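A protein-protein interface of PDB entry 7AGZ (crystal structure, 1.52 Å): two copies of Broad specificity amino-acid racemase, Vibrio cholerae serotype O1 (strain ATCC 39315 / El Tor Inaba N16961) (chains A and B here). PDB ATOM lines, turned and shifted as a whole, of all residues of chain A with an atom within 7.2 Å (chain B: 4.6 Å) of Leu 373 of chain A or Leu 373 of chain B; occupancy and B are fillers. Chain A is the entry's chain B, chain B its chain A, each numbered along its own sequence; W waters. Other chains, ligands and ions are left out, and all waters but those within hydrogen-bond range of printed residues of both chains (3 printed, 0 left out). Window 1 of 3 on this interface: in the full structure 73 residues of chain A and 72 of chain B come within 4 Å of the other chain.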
ATOM      1  N   LEU A  22       9.215   8.861   4.764  1.00  0.00           N
ATOM      2  CA  LEU A  22       7.840   8.366   4.828  1.00  0.00           C
ATOM      3  C   LEU A  22       7.410   8.194   6.274  1.00  0.00           C
ATOM      4  O   LEU A  22       8.187   7.735   7.110  1.00  0.00           O
ATOM      5  CB  LEU A  22       7.718   7.034   4.114  1.00  0.00           C
ATOM      6  CG  LEU A  22       8.052   7.044   2.635  1.00  0.00           C
ATOM      7  CD1 LEU A  22       7.839   5.616   2.081  1.00  0.00           C
ATOM      8  CD2 LEU A  22       7.226   8.031   1.842  1.00  0.00           C
ATOM      9  N   ALA A  52       6.721  -6.053  -2.755  1.00  0.00           N
ATOM     10  CA  ALA A  52       7.384  -4.744  -2.857  1.00  0.00           C
ATOM     11  C   ALA A  52       7.551  -4.073  -1.485  1.00  0.00           C
ATOM     12  O   ALA A  52       7.265  -2.879  -1.300  1.00  0.00           O
ATOM     13  CB  ALA A  52       6.645  -3.835  -3.838  1.00  0.00           C
ATOM     14  N   TYR A  55       4.288  -2.930  -0.111  1.00  0.00           N
ATOM     15  CA  TYR A  55       3.773  -1.813  -0.894  1.00  0.00           C
ATOM     16  C   TYR A  55       4.474  -0.513  -0.519  1.00  0.00           C
ATOM     17  O   TYR A  55       3.862   0.553  -0.506  1.00  0.00           O
ATOM     18  CB  TYR A  55       2.249  -1.694  -0.775  1.00  0.00           C
ATOM     19  CG  TYR A  55       1.458  -2.739  -1.585  1.00  0.00           C
ATOM     20  CD1 TYR A  55       1.779  -4.121  -1.523  1.00  0.00           C
ATOM     21  CD2 TYR A  55       0.376  -2.344  -2.403  1.00  0.00           C
ATOM     22  CE1 TYR A  55       1.014  -5.088  -2.248  1.00  0.00           C
ATOM     23  CE2 TYR A  55      -0.381  -3.308  -3.119  1.00  0.00           C
ATOM     24  CZ  TYR A  55      -0.032  -4.661  -3.030  1.00  0.00           C
ATOM     25  OH  TYR A  55      -0.789  -5.583  -3.713  1.00  0.00           O
ATOM     26  N   GLY A  56       5.786  -0.611  -0.282  1.00  0.00           N
ATOM     27  CA  GLY A  56       6.600   0.539   0.091  1.00  0.00           C
ATOM     28  C   GLY A  56       6.546   0.876   1.556  1.00  0.00           C
ATOM     29  O   GLY A  56       7.300   1.758   2.019  1.00  0.00           O
ATOM     30  N   GLY A 294      13.915  15.582  -4.471  1.00  0.00           N
ATOM     31  CA  GLY A 294      13.800  15.631  -5.917  1.00  0.00           C
ATOM     32  C   GLY A 294      13.432  14.299  -6.519  1.00  0.00           C
ATOM     33  O   GLY A 294      12.950  13.404  -5.809  1.00  0.00           O
ATOM     34  N   TYR A 295      13.666  14.143  -7.830  1.00  0.00           N
ATOM     35  CA  TYR A 295      13.172  12.928  -8.475  1.00  0.00           C
ATOM     36  C   TYR A 295      13.967  11.701  -8.054  1.00  0.00           C
ATOM     37  O   TYR A 295      13.417  10.591  -8.142  1.00  0.00           O
ATOM     38  CB  TYR A 295      13.069  13.110  -9.996  1.00  0.00           C
ATOM     39  CG  TYR A 295      14.349  13.436 -10.750  1.00  0.00           C
ATOM     40  CD1 TYR A 295      15.363  12.496 -10.928  1.00  0.00           C
ATOM     41  CD2 TYR A 295      14.489  14.722 -11.318  1.00  0.00           C
ATOM     42  CE1 TYR A 295      16.533  12.803 -11.633  1.00  0.00           C
ATOM     43  CE2 TYR A 295      15.641  15.025 -12.046  1.00  0.00           C
ATOM     44  CZ  TYR A 295      16.633  14.067 -12.179  1.00  0.00           C
ATOM     45  OH  TYR A 295      17.736  14.443 -12.885  1.00  0.00           O
ATOM     46  N   SER A 296      15.204  11.866  -7.550  1.00  0.00           N
ATOM     47  CA  SER A 296      15.975  10.748  -6.994  1.00  0.00           C
ATOM     48  C   SER A 296      15.376  10.186  -5.697  1.00  0.00           C
ATOM     49  O   SER A 296      15.813   9.125  -5.213  1.00  0.00           O
ATOM     50  CB  SER A 296      17.448  11.164  -6.802  1.00  0.00           C
ATOM     51  OG  SER A 296      17.583  12.073  -5.719  1.00  0.00           O
ATOM     52  N   ASP A 297      14.487  10.944  -5.052  1.00  0.00           N
ATOM     53  CA  ASP A 297      13.749  10.494  -3.876  1.00  0.00           C
ATOM     54  C   ASP A 297      12.378   9.980  -4.229  1.00  0.00           C
ATOM     55  O   ASP A 297      11.627   9.572  -3.320  1.00  0.00           O
ATOM     56  CB  ASP A 297      13.627  11.645  -2.854  1.00  0.00           C
ATOM     57  CG  ASP A 297      14.967  12.296  -2.547  1.00  0.00           C
ATOM     58  OD1 ASP A 297      15.786  11.629  -1.880  1.00  0.00           O
ATOM     59  OD2 ASP A 297      15.195  13.430  -3.038  1.00  0.00           O
ATOM     60  N   GLY A 298      12.010  10.031  -5.502  1.00  0.00           N
ATOM     61  CA  GLY A 298      10.696   9.610  -5.949  1.00  0.00           C
ATOM     62  C   GLY A 298       9.674  10.732  -6.086  1.00  0.00           C
ATOM     63  O   GLY A 298       8.492  10.429  -6.246  1.00  0.00           O
ATOM     64  N   TYR A 299      10.107  12.031  -6.109  1.00  0.00           N
ATOM     65  CA  TYR A 299       9.190  13.130  -6.397  1.00  0.00           C
ATOM     66  C   TYR A 299       9.375  13.541  -7.866  1.00  0.00           C
ATOM     67  O   TYR A 299      10.369  14.196  -8.206  1.00  0.00           O
ATOM     68  CB  TYR A 299       9.444  14.290  -5.440  1.00  0.00           C
ATOM     69  CG  TYR A 299       8.306  15.280  -5.404  1.00  0.00           C
ATOM     70  CD1 TYR A 299       7.087  14.923  -4.845  1.00  0.00           C
ATOM     71  CD2 TYR A 299       8.463  16.577  -5.883  1.00  0.00           C
ATOM     72  CE1 TYR A 299       6.014  15.821  -4.811  1.00  0.00           C
ATOM     73  CE2 TYR A 299       7.404  17.497  -5.847  1.00  0.00           C
ATOM     74  CZ  TYR A 299       6.180  17.091  -5.279  1.00  0.00           C
ATOM     75  OH  TYR A 299       5.145  17.949  -5.260  1.00  0.00           O
ATOM     76  N   PRO A 300       8.492  13.142  -8.785  1.00  0.00           N
ATOM     77  CA  PRO A 300       8.850  13.206 -10.210  1.00  0.00           C
ATOM     78  C   PRO A 300       9.083  14.607 -10.769  1.00  0.00           C
ATOM     79  O   PRO A 300       8.594  15.623 -10.287  1.00  0.00           O
ATOM     80  CB  PRO A 300       7.644  12.549 -10.905  1.00  0.00           C
ATOM     81  CG  PRO A 300       7.074  11.679  -9.857  1.00  0.00           C
ATOM     82  CD  PRO A 300       7.243  12.386  -8.564  1.00  0.00           C
ATOM     83  N   LEU A 365       1.256   9.016 -13.377  1.00  0.00           N
ATOM     84  CA  LEU A 365       1.572   7.655 -12.966  1.00  0.00           C
ATOM     85  C   LEU A 365       0.385   7.109 -12.192  1.00  0.00           C
ATOM     86  O   LEU A 365      -0.475   7.869 -11.752  1.00  0.00           O
ATOM     87  CB  LEU A 365       2.771   7.642 -12.028  1.00  0.00           C
ATOM     88  CG  LEU A 365       4.107   8.118 -12.533  1.00  0.00           C
ATOM     89  CD1 LEU A 365       5.096   8.129 -11.369  1.00  0.00           C
ATOM     90  CD2 LEU A 365       4.608   7.230 -13.688  1.00  0.00           C
ATOM     91  N   PHE A 367      -0.860   5.444  -8.638  1.00  0.00           N
ATOM     92  CA  PHE A 367      -0.350   5.650  -7.273  1.00  0.00           C
ATOM     93  C   PHE A 367       0.720   4.639  -6.850  1.00  0.00           C
ATOM     94  O   PHE A 367       1.737   5.058  -6.265  1.00  0.00           O
ATOM     95  CB  PHE A 367      -1.565   5.684  -6.317  1.00  0.00           C
ATOM     96  CG  PHE A 367      -1.275   6.088  -4.873  1.00  0.00           C
ATOM     97  CD1 PHE A 367      -0.370   7.101  -4.563  1.00  0.00           C
ATOM     98  CD2 PHE A 367      -2.021   5.490  -3.857  1.00  0.00           C
ATOM     99  CE1 PHE A 367      -0.149   7.469  -3.195  1.00  0.00           C
ATOM    100  CE2 PHE A 367      -1.824   5.827  -2.534  1.00  0.00           C
ATOM    101  CZ  PHE A 367      -0.849   6.813  -2.214  1.00  0.00           C
ATOM    102  N   PRO A 368       0.569   3.332  -7.074  1.00  0.00           N
ATOM    103  CA  PRO A 368       1.619   2.397  -6.622  1.00  0.00           C
ATOM    104  C   PRO A 368       2.950   2.591  -7.337  1.00  0.00           C
ATOM    105  O   PRO A 368       3.970   2.195  -6.776  1.00  0.00           O
ATOM    106  CB  PRO A 368       1.038   0.995  -6.922  1.00  0.00           C
ATOM    107  CG  PRO A 368      -0.126   1.227  -7.830  1.00  0.00           C
ATOM    108  CD  PRO A 368      -0.619   2.613  -7.583  1.00  0.00           C
ATOM    109  N   GLU A 369       2.960   3.153  -8.542  1.00  0.00           N
ATOM    110  CA  GLU A 369       4.249   3.450  -9.177  1.00  0.00           C
ATOM    111  C   GLU A 369       5.036   4.452  -8.350  1.00  0.00           C
ATOM    112  O   GLU A 369       6.270   4.398  -8.298  1.00  0.00           O
ATOM    113  CB  GLU A 369       4.058   3.964 -10.603  1.00  0.00           C
ATOM    114  CG  GLU A 369       3.663   2.894 -11.624  1.00  0.00           C
ATOM    115  CD  GLU A 369       3.532   3.508 -12.968  1.00  0.00           C
ATOM    116  OE1 GLU A 369       2.489   4.121 -13.251  1.00  0.00           O
ATOM    117  OE2 GLU A 369       4.519   3.478 -13.711  1.00  0.00           O
ATOM    118  N   LEU A 370       4.343   5.392  -7.724  1.00  0.00           N
ATOM    119  CA  LEU A 370       4.982   6.343  -6.811  1.00  0.00           C
ATOM    120  C   LEU A 370       5.411   5.687  -5.489  1.00  0.00           C
ATOM    121  O   LEU A 370       6.586   5.725  -5.101  1.00  0.00           O
ATOM    122  CB  LEU A 370       4.000   7.494  -6.517  1.00  0.00           C
ATOM    123  CG  LEU A 370       3.814   8.491  -7.668  1.00  0.00           C
ATOM    124  CD1 LEU A 370       2.535   9.338  -7.499  1.00  0.00           C
ATOM    125  CD2 LEU A 370       5.085   9.341  -7.891  1.00  0.00           C
ATOM    126  N   TYR A 371       4.469   5.066  -4.783  1.00  0.00           N
ATOM    127  CA  TYR A 371       4.771   4.705  -3.404  1.00  0.00           C
ATOM    128  C   TYR A 371       5.712   3.512  -3.299  1.00  0.00           C
ATOM    129  O   TYR A 371       6.450   3.424  -2.313  1.00  0.00           O
ATOM    130  CB  TYR A 371       3.475   4.513  -2.568  1.00  0.00           C
ATOM    131  CG  TYR A 371       2.439   3.454  -2.925  1.00  0.00           C
ATOM    132  CD1 TYR A 371       2.737   2.083  -2.928  1.00  0.00           C
ATOM    133  CD2 TYR A 371       1.122   3.843  -3.179  1.00  0.00           C
ATOM    134  CE1 TYR A 371       1.757   1.149  -3.219  1.00  0.00           C
ATOM    135  CE2 TYR A 371       0.132   2.899  -3.482  1.00  0.00           C
ATOM    136  CZ  TYR A 371       0.466   1.572  -3.495  1.00  0.00           C
ATOM    137  OH  TYR A 371      -0.467   0.597  -3.776  1.00  0.00           O
ATOM    138  N   THR A 372       5.754   2.602  -4.286  1.00  0.00           N
ATOM    139  CA  THR A 372       6.713   1.507  -4.169  1.00  0.00           C
ATOM    140  C   THR A 372       8.143   2.034  -4.262  1.00  0.00           C
ATOM    141  O   THR A 372       9.038   1.556  -3.547  1.00  0.00           O
ATOM    142  CB  THR A 372       6.433   0.413  -5.224  1.00  0.00           C
ATOM    143  OG1 THR A 372       6.462   0.959  -6.555  1.00  0.00           O
ATOM    144  CG2 THR A 372       5.104  -0.322  -4.945  1.00  0.00           C
ATOM    145  N   LEU A 373       8.376   3.042  -5.108  1.00  0.00           N
ATOM    146  CA  LEU A 373       9.716   3.617  -5.211  1.00  0.00           C
ATOM    147  C   LEU A 373       9.974   4.647  -4.096  1.00  0.00           C
ATOM    148  O   LEU A 373      11.136   4.882  -3.719  1.00  0.00           O
ATOM    149  CB  LEU A 373       9.943   4.209  -6.609  1.00  0.00           C
ATOM    150  CG  LEU A 373       9.808   3.163  -7.734  1.00  0.00           C
ATOM    151  CD1 LEU A 373      10.023   3.753  -9.088  1.00  0.00           C
ATOM    152  CD2 LEU A 373      10.808   2.023  -7.489  1.00  0.00           C
ATOM    153  N   TRP A 374       8.927   5.295  -3.552  1.00  0.00           N
ATOM    154  CA  TRP A 374       9.168   6.055  -2.322  1.00  0.00           C
ATOM    155  C   TRP A 374       9.794   5.151  -1.287  1.00  0.00           C
ATOM    156  O   TRP A 374      10.679   5.562  -0.540  1.00  0.00           O
ATOM    157  CB  TRP A 374       7.893   6.631  -1.707  1.00  0.00           C
ATOM    158  CG  TRP A 374       7.262   7.655  -2.520  1.00  0.00           C
ATOM    159  CD1 TRP A 374       7.807   8.317  -3.597  1.00  0.00           C
ATOM    160  CD2 TRP A 374       5.921   8.133  -2.387  1.00  0.00           C
ATOM    161  NE1 TRP A 374       6.875   9.176  -4.137  1.00  0.00           N
ATOM    162  CE2 TRP A 374       5.713   9.094  -3.412  1.00  0.00           C
ATOM    163  CE3 TRP A 374       4.868   7.841  -1.494  1.00  0.00           C
ATOM    164  CZ2 TRP A 374       4.517   9.762  -3.587  1.00  0.00           C
ATOM    165  CZ3 TRP A 374       3.670   8.535  -1.652  1.00  0.00           C
ATOM    166  CH2 TRP A 374       3.503   9.476  -2.687  1.00  0.00           C
ATOM    167  N   GLY A 375       9.283   3.909  -1.186  1.00  0.00           N
ATOM    168  CA  GLY A 375       9.728   3.014  -0.135  1.00  0.00           C
ATOM    169  C   GLY A 375      11.133   2.460  -0.291  1.00  0.00           C
ATOM    170  O   GLY A 375      11.738   2.027   0.694  1.00  0.00           O
ATOM    171  N   THR A 376      11.633   2.338  -1.526  1.00  0.00           N
ATOM    172  CA  THR A 376      13.028   1.928  -1.683  1.00  0.00           C
ATOM    173  C   THR A 376      14.005   3.085  -1.528  1.00  0.00           C
ATOM    174  O   THR A 376      15.210   2.850  -1.368  1.00  0.00           O
ATOM    175  CB  THR A 376      13.271   1.296  -3.054  1.00  0.00           C
ATOM    176  OG1 THR A 376      12.899   2.227  -4.076  1.00  0.00           O
ATOM    177  CG2 THR A 376      12.471   0.001  -3.247  1.00  0.00           C
ATOM    178  N   SER A 377      13.512   4.328  -1.547  1.00  0.00           N
ATOM    179  CA  SER A 377      14.433   5.449  -1.670  1.00  0.00           C
ATOM    180  C   SER A 377      14.366   6.427  -0.520  1.00  0.00           C
ATOM    181  O   SER A 377      15.049   7.438  -0.567  1.00  0.00           O
ATOM    182  CB  SER A 377      14.190   6.227  -2.973  1.00  0.00           C
ATOM    183  OG  SER A 377      13.883   5.363  -4.096  1.00  0.00           O
ATOM    184  N   ASN A 378      13.653   6.104   0.555  1.00  0.00           N
ATOM    185  CA  ASN A 378      13.517   7.004   1.705  1.00  0.00           C
ATOM    186  C   ASN A 378      13.333   6.151   2.946  1.00  0.00           C
ATOM    187  O   ASN A 378      12.699   5.085   2.859  1.00  0.00           O
ATOM    188  CB  ASN A 378      12.268   7.903   1.570  1.00  0.00           C
ATOM    189  CG  ASN A 378      12.310   8.786   0.348  1.00  0.00           C
ATOM    190  OD1 ASN A 378      12.955   9.834   0.370  1.00  0.00           O
ATOM    191  ND2 ASN A 378      11.657   8.347  -0.743  1.00  0.00           N
ATOM    192  N   TYR B 295       7.247  -2.494 -12.039  1.00  0.00           N
ATOM    193  CA  TYR B 295       7.476  -1.062 -11.780  1.00  0.00           C
ATOM    194  C   TYR B 295       8.051  -0.802 -10.390  1.00  0.00           C
ATOM    195  O   TYR B 295       8.672   0.249 -10.168  1.00  0.00           O
ATOM    196  CB  TYR B 295       6.211  -0.230 -12.080  1.00  0.00           C
ATOM    197  CG  TYR B 295       4.957  -0.551 -11.304  1.00  0.00           C
ATOM    198  CD1 TYR B 295       4.837  -0.249  -9.950  1.00  0.00           C
ATOM    199  CD2 TYR B 295       3.865  -1.114 -11.952  1.00  0.00           C
ATOM    200  CE1 TYR B 295       3.686  -0.580  -9.262  1.00  0.00           C
ATOM    201  CE2 TYR B 295       2.700  -1.387 -11.276  1.00  0.00           C
ATOM    202  CZ  TYR B 295       2.615  -1.112  -9.937  1.00  0.00           C
ATOM    203  OH  TYR B 295       1.443  -1.442  -9.277  1.00  0.00           O
ATOM    204  N   SER B 296       7.887  -1.721  -9.442  1.00  0.00           N
ATOM    205  CA  SER B 296       8.516  -1.572  -8.121  1.00  0.00           C
ATOM    206  C   SER B 296      10.028  -1.742  -8.137  1.00  0.00           C
ATOM    207  O   SER B 296      10.683  -1.467  -7.110  1.00  0.00           O
ATOM    208  CB  SER B 296       7.879  -2.540  -7.116  1.00  0.00           C
ATOM    209  OG  SER B 296       7.833  -3.888  -7.597  1.00  0.00           O
ATOM    210  N   ASP B 297      10.558  -2.265  -9.232  1.00  0.00           N
ATOM    211  CA  ASP B 297      11.989  -2.346  -9.465  1.00  0.00           C
ATOM    212  C   ASP B 297      12.462  -1.183 -10.300  1.00  0.00           C
ATOM    213  O   ASP B 297      13.652  -1.113 -10.610  1.00  0.00           O
ATOM    214  CB  ASP B 297      12.327  -3.670 -10.192  1.00  0.00           C
ATOM    215  CG  ASP B 297      11.702  -4.879  -9.506  1.00  0.00           C
ATOM    216  OD1 ASP B 297      12.153  -5.222  -8.404  1.00  0.00           O
ATOM    217  OD2 ASP B 297      10.738  -5.492 -10.026  1.00  0.00           O
ATOM    218  N   GLY B 298      11.558  -0.323 -10.729  1.00  0.00           N
ATOM    219  CA  GLY B 298      11.900   0.799 -11.571  1.00  0.00           C
ATOM    220  C   GLY B 298      11.741   0.584 -13.057  1.00  0.00           C
ATOM    221  O   GLY B 298      12.290   1.391 -13.835  1.00  0.00           O
ATOM    222  N   GLU B 369      15.685  10.115 -14.251  1.00  0.00           N
ATOM    223  CA  GLU B 369      14.545   9.714 -13.427  1.00  0.00           C
ATOM    224  C   GLU B 369      14.471   8.193 -13.325  1.00  0.00           C
ATOM    225  O   GLU B 369      13.980   7.647 -12.319  1.00  0.00           O
ATOM    226  CB  GLU B 369      13.257  10.259 -14.016  1.00  0.00           C
ATOM    227  CG  GLU B 369      13.048  11.759 -13.835  1.00  0.00           C
ATOM    228  CD  GLU B 369      11.735  12.189 -14.416  1.00  0.00           C
ATOM    229  OE1 GLU B 369      11.645  12.369 -15.656  1.00  0.00           O
ATOM    230  OE2 GLU B 369      10.750  12.286 -13.620  1.00  0.00           O
ATOM    231  N   LEU B 370      14.838   7.503 -14.395  1.00  0.00           N
ATOM    232  CA  LEU B 370      14.903   6.039 -14.359  1.00  0.00           C
ATOM    233  C   LEU B 370      16.092   5.558 -13.525  1.00  0.00           C
ATOM    234  O   LEU B 370      15.937   4.837 -12.533  1.00  0.00           O
ATOM    235  CB  LEU B 370      15.034   5.502 -15.799  1.00  0.00           C
ATOM    236  CG  LEU B 370      13.747   5.590 -16.619  1.00  0.00           C
ATOM    237  CD1 LEU B 370      13.963   5.472 -18.129  1.00  0.00           C
ATOM    238  CD2 LEU B 370      12.810   4.497 -16.108  1.00  0.00           C
ATOM    239  N   TYR B 371      17.308   5.990 -13.883  1.00  0.00           N
ATOM    240  CA  TYR B 371      18.444   5.285 -13.305  1.00  0.00           C
ATOM    241  C   TYR B 371      18.689   5.601 -11.838  1.00  0.00           C
ATOM    242  O   TYR B 371      19.258   4.761 -11.117  1.00  0.00           O
ATOM    243  CB  TYR B 371      19.682   5.480 -14.182  1.00  0.00           C
ATOM    244  CG  TYR B 371      20.239   6.880 -14.425  1.00  0.00           C
ATOM    245  CD1 TYR B 371      20.705   7.690 -13.379  1.00  0.00           C
ATOM    246  CD2 TYR B 371      20.423   7.319 -15.735  1.00  0.00           C
ATOM    247  CE1 TYR B 371      21.251   8.947 -13.634  1.00  0.00           C
ATOM    248  CE2 TYR B 371      20.998   8.549 -16.025  1.00  0.00           C
ATOM    249  CZ  TYR B 371      21.419   9.355 -14.975  1.00  0.00           C
ATOM    250  OH  TYR B 371      21.981  10.613 -15.126  1.00  0.00           O
ATOM    251  N   THR B 372      18.289   6.783 -11.354  1.00  0.00           N
ATOM    252  CA  THR B 372      18.485   7.046  -9.928  1.00  0.00           C
ATOM    253  C   THR B 372      17.610   6.113  -9.089  1.00  0.00           C
ATOM    254  O   THR B 372      18.029   5.691  -8.002  1.00  0.00           O
ATOM    255  CB  THR B 372      18.232   8.520  -9.567  1.00  0.00           C
ATOM    256  OG1 THR B 372      16.898   8.951  -9.930  1.00  0.00           O
ATOM    257  CG2 THR B 372      19.315   9.470 -10.141  1.00  0.00           C
ATOM    258  N   LEU B 373      16.409   5.792  -9.577  1.00  0.00           N
ATOM    259  CA  LEU B 373      15.528   4.881  -8.825  1.00  0.00           C
ATOM    260  C   LEU B 373      15.876   3.416  -9.073  1.00  0.00           C
ATOM    261  O   LEU B 373      15.678   2.564  -8.203  1.00  0.00           O
ATOM    262  CB  LEU B 373      14.052   5.184  -9.120  1.00  0.00           C
ATOM    263  CG  LEU B 373      13.679   6.636  -8.726  1.00  0.00           C
ATOM    264  CD1 LEU B 373      12.187   6.937  -9.010  1.00  0.00           C
ATOM    265  CD2 LEU B 373      13.978   6.945  -7.264  1.00  0.00           C
ATOM    266  N   TRP B 374      16.453   3.091 -10.232  1.00  0.00           N
ATOM    267  CA  TRP B 374      17.036   1.749 -10.378  1.00  0.00           C
ATOM    268  C   TRP B 374      18.031   1.485  -9.266  1.00  0.00           C
ATOM    269  O   TRP B 374      18.086   0.385  -8.697  1.00  0.00           O
ATOM    270  CB  TRP B 374      17.790   1.592 -11.714  1.00  0.00           C
ATOM    271  CG  TRP B 374      16.931   1.625 -12.930  1.00  0.00           C
ATOM    272  CD1 TRP B 374      15.538   1.505 -12.977  1.00  0.00           C
ATOM    273  CD2 TRP B 374      17.368   1.800 -14.291  1.00  0.00           C
ATOM    274  NE1 TRP B 374      15.114   1.571 -14.294  1.00  0.00           N
ATOM    275  CE2 TRP B 374      16.209   1.772 -15.108  1.00  0.00           C
ATOM    276  CE3 TRP B 374      18.639   1.976 -14.889  1.00  0.00           C
ATOM    277  CZ2 TRP B 374      16.257   1.946 -16.486  1.00  0.00           C
ATOM    278  CZ3 TRP B 374      18.688   2.133 -16.296  1.00  0.00           C
ATOM    279  CH2 TRP B 374      17.495   2.105 -17.068  1.00  0.00           C
ATOM    280  N   GLY B 375      18.849   2.493  -8.964  1.00  0.00           N
ATOM    281  CA  GLY B 375      19.909   2.307  -8.004  1.00  0.00           C
ATOM    282  C   GLY B 375      19.461   2.162  -6.564  1.00  0.00           C
ATOM    283  O   GLY B 375      20.150   1.513  -5.768  1.00  0.00           O
ATOM    284  N   THR B 376      18.312   2.756  -6.196  1.00  0.00           N
ATOM    285  CA  THR B 376      17.801   2.533  -4.852  1.00  0.00           C
ATOM    286  C   THR B 376      17.022   1.238  -4.717  1.00  0.00           C
ATOM    287  O   THR B 376      16.767   0.794  -3.582  1.00  0.00           O
ATOM    288  CB  THR B 376      16.892   3.668  -4.414  1.00  0.00           C
ATOM    289  OG1 THR B 376      15.813   3.792  -5.342  1.00  0.00           O
ATOM    290  CG2 THR B 376      17.658   5.037  -4.317  1.00  0.00           C
ATOM    291  N   SER B 377      16.654   0.599  -5.854  1.00  0.00           N
ATOM    292  CA  SER B 377      15.677  -0.492  -5.845  1.00  0.00           C
ATOM    293  C   SER B 377      16.230  -1.805  -6.344  1.00  0.00           C
ATOM    294  O   SER B 377      15.469  -2.779  -6.431  1.00  0.00           O
ATOM    295  CB  SER B 377      14.476  -0.112  -6.712  1.00  0.00           C
ATOM    296  OG  SER B 377      13.969   1.183  -6.346  1.00  0.00           O
HETATM  297  O   HOH W   1      12.887   9.614 -10.671  1.00  0.00           O
HETATM  298  O   HOH W   2      16.787   0.922  -1.183  1.00  0.00           O
HETATM  299  O   HOH W   3       7.169   2.559 -10.277  1.00  0.00           O
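OG of Ser 377 of chain B sits at hydrogen-bond distance from OG1 of Thr 376 of chain A (2.7 Å). OG1 of Thr 376 of chain B lies within hydrogen-bond range of OG of Ser 377 of chain A, at 2.8 Å. O of Thr 376 of chain A sits close to O of Thr 376 of chain B, 3.4 Å away.
OG1 of Thr 376 of chain B is in hydrogen-bond range of OG of Ser 377 of chain B, at 3.3 Å. The side-chain hydroxyl (OG1) of Thr 376 of chain A is in hydrogen-bond range of the side-chain hydroxyl (OG) of Ser 377 of chain A, at 3.3 Å. O of Leu 373 of chain A sits at hydrogen-bond distance from OG1 of Thr 376 of chain A, 3.2 Å away. O of Pro 368 of chain A lies within hydrogen-bond range of OG1 of Thr 372 of chain A (2.8 Å). The backbone carbonyl oxygen (O) of Leu 373 of chain A lies within hydrogen-bond range of the side-chain hydroxyl (OG) of Ser 377 of chain A, 2.8 Å away.
Ser 296 of chain B touches Ala 52 of chain A (CB to CB, 3.7 Å). CG of Tyr 295 of chain A touches CG of Glu 369 of chain B, at 3.7 Å. Tyr 295 of chain A touches Thr 372 of chain B. Tyr 295 of chain A touches Leu 373 of chain B (O to CD2, 3.8 Å). Ser 296 of chain A touches Leu 373 of chain B (O to CD2, 3.5 Å). CD1 of Tyr 295 of chain B touches OG1 of Thr 372 of chain A, at 3.95 Å. Thr 372 of chain A touches Ser 296 of chain B (OG1 to CA, 3.6 Å). O of Ser 296 of chain B touches CD2 of Leu 373 of chain A, 3.5 Å away. Leu 373 of chain A touches Ser 377 of chain B (CD2 to OG, 3.5 Å).
Of the printed residues of chain B, Leu 373 of chain A touches Tyr 295, Ser 296, Leu 373 and Ser 377. Printed residues of chain A within 4 Å of Leu 373 of chain B: Tyr 295 (3.8 Å), Ser 296 (3.5 Å), Leu 373 (3.9 Å) and Ser 377 (3.5 Å). Of the printed residues of chain B, Ser 377 of chain A touches Leu 373 and Thr 376. Of the printed residues of chain B, Pro 368 of chain A touches Tyr 295. Of the printed residues of chain A, Glu 369 of chain B touches Tyr 295. Asp 297 of chain A touches none of the printed residues of chain B. The nearest residue of chain B that does not touch Leu 373 of chain A is Gly 298 of chain B (4.1 Å). The nearest printed residue of chain B that does not touch Ser 296 of chain A is Thr 376 of chain B (4.6 Å).
Of the 13 printed residues of chain B, 7 touch a printed residue of chain A. Hydrophobic or aromatic side chains of chain B within 4 Å of the printed part of chain A: Tyr 295 and Leu 373. Of the 24 printed residues of chain A, 9 touch a printed residue of chain B. Printed residues of chain A that touch a printed residue of chain B: Ala 52, Tyr 295, Ser 296, Pro 368, Glu 369, Thr 372, Leu 373, Thr 376 and Ser 377. Among the printed residues, no Asp or Glu carboxylate lies within 4 Å of a Lys or Arg side-chain nitrogen of the other chain.
Tyr 295 of chain A touches Glu 369 of chain B, and with the chains exchanged Glu 369 of chain A touches Tyr 295 of chain B. Tyr 295 of chain A touches Thr 372 of chain B, and with the chains exchanged Thr 372 of chain A touches Tyr 295 of chain B. Tyr 295 of chain A touches Leu 373 of chain B, and with the chains exchanged Leu 373 of chain A touches Tyr 295 of chain B. Thr 376 of chain B touches its own counterpart, Thr 376 of chain A. Positions printed for both chains: 295, 296, 297, 298, 369, 370, 371, 372, 373, 374, 375, 376 and 377.
Water W2 lies within hydrogen-bond range of O of Thr 376 of chain B and O of Thr 376 of chain A. Water W3 bridges the backbone carbonyl oxygen (O) of Tyr 295 of chain B (2.8 Å) and the backbone carbonyl oxygen (O) of Glu 369 of chain A (2.8 Å). Water W1 lies within hydrogen-bond range of the backbone carbonyl oxygen (O) of Tyr 295 of chain A (2.8 Å) and the backbone carbonyl oxygen (O) of Glu 369 of chain B (2.8 Å).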
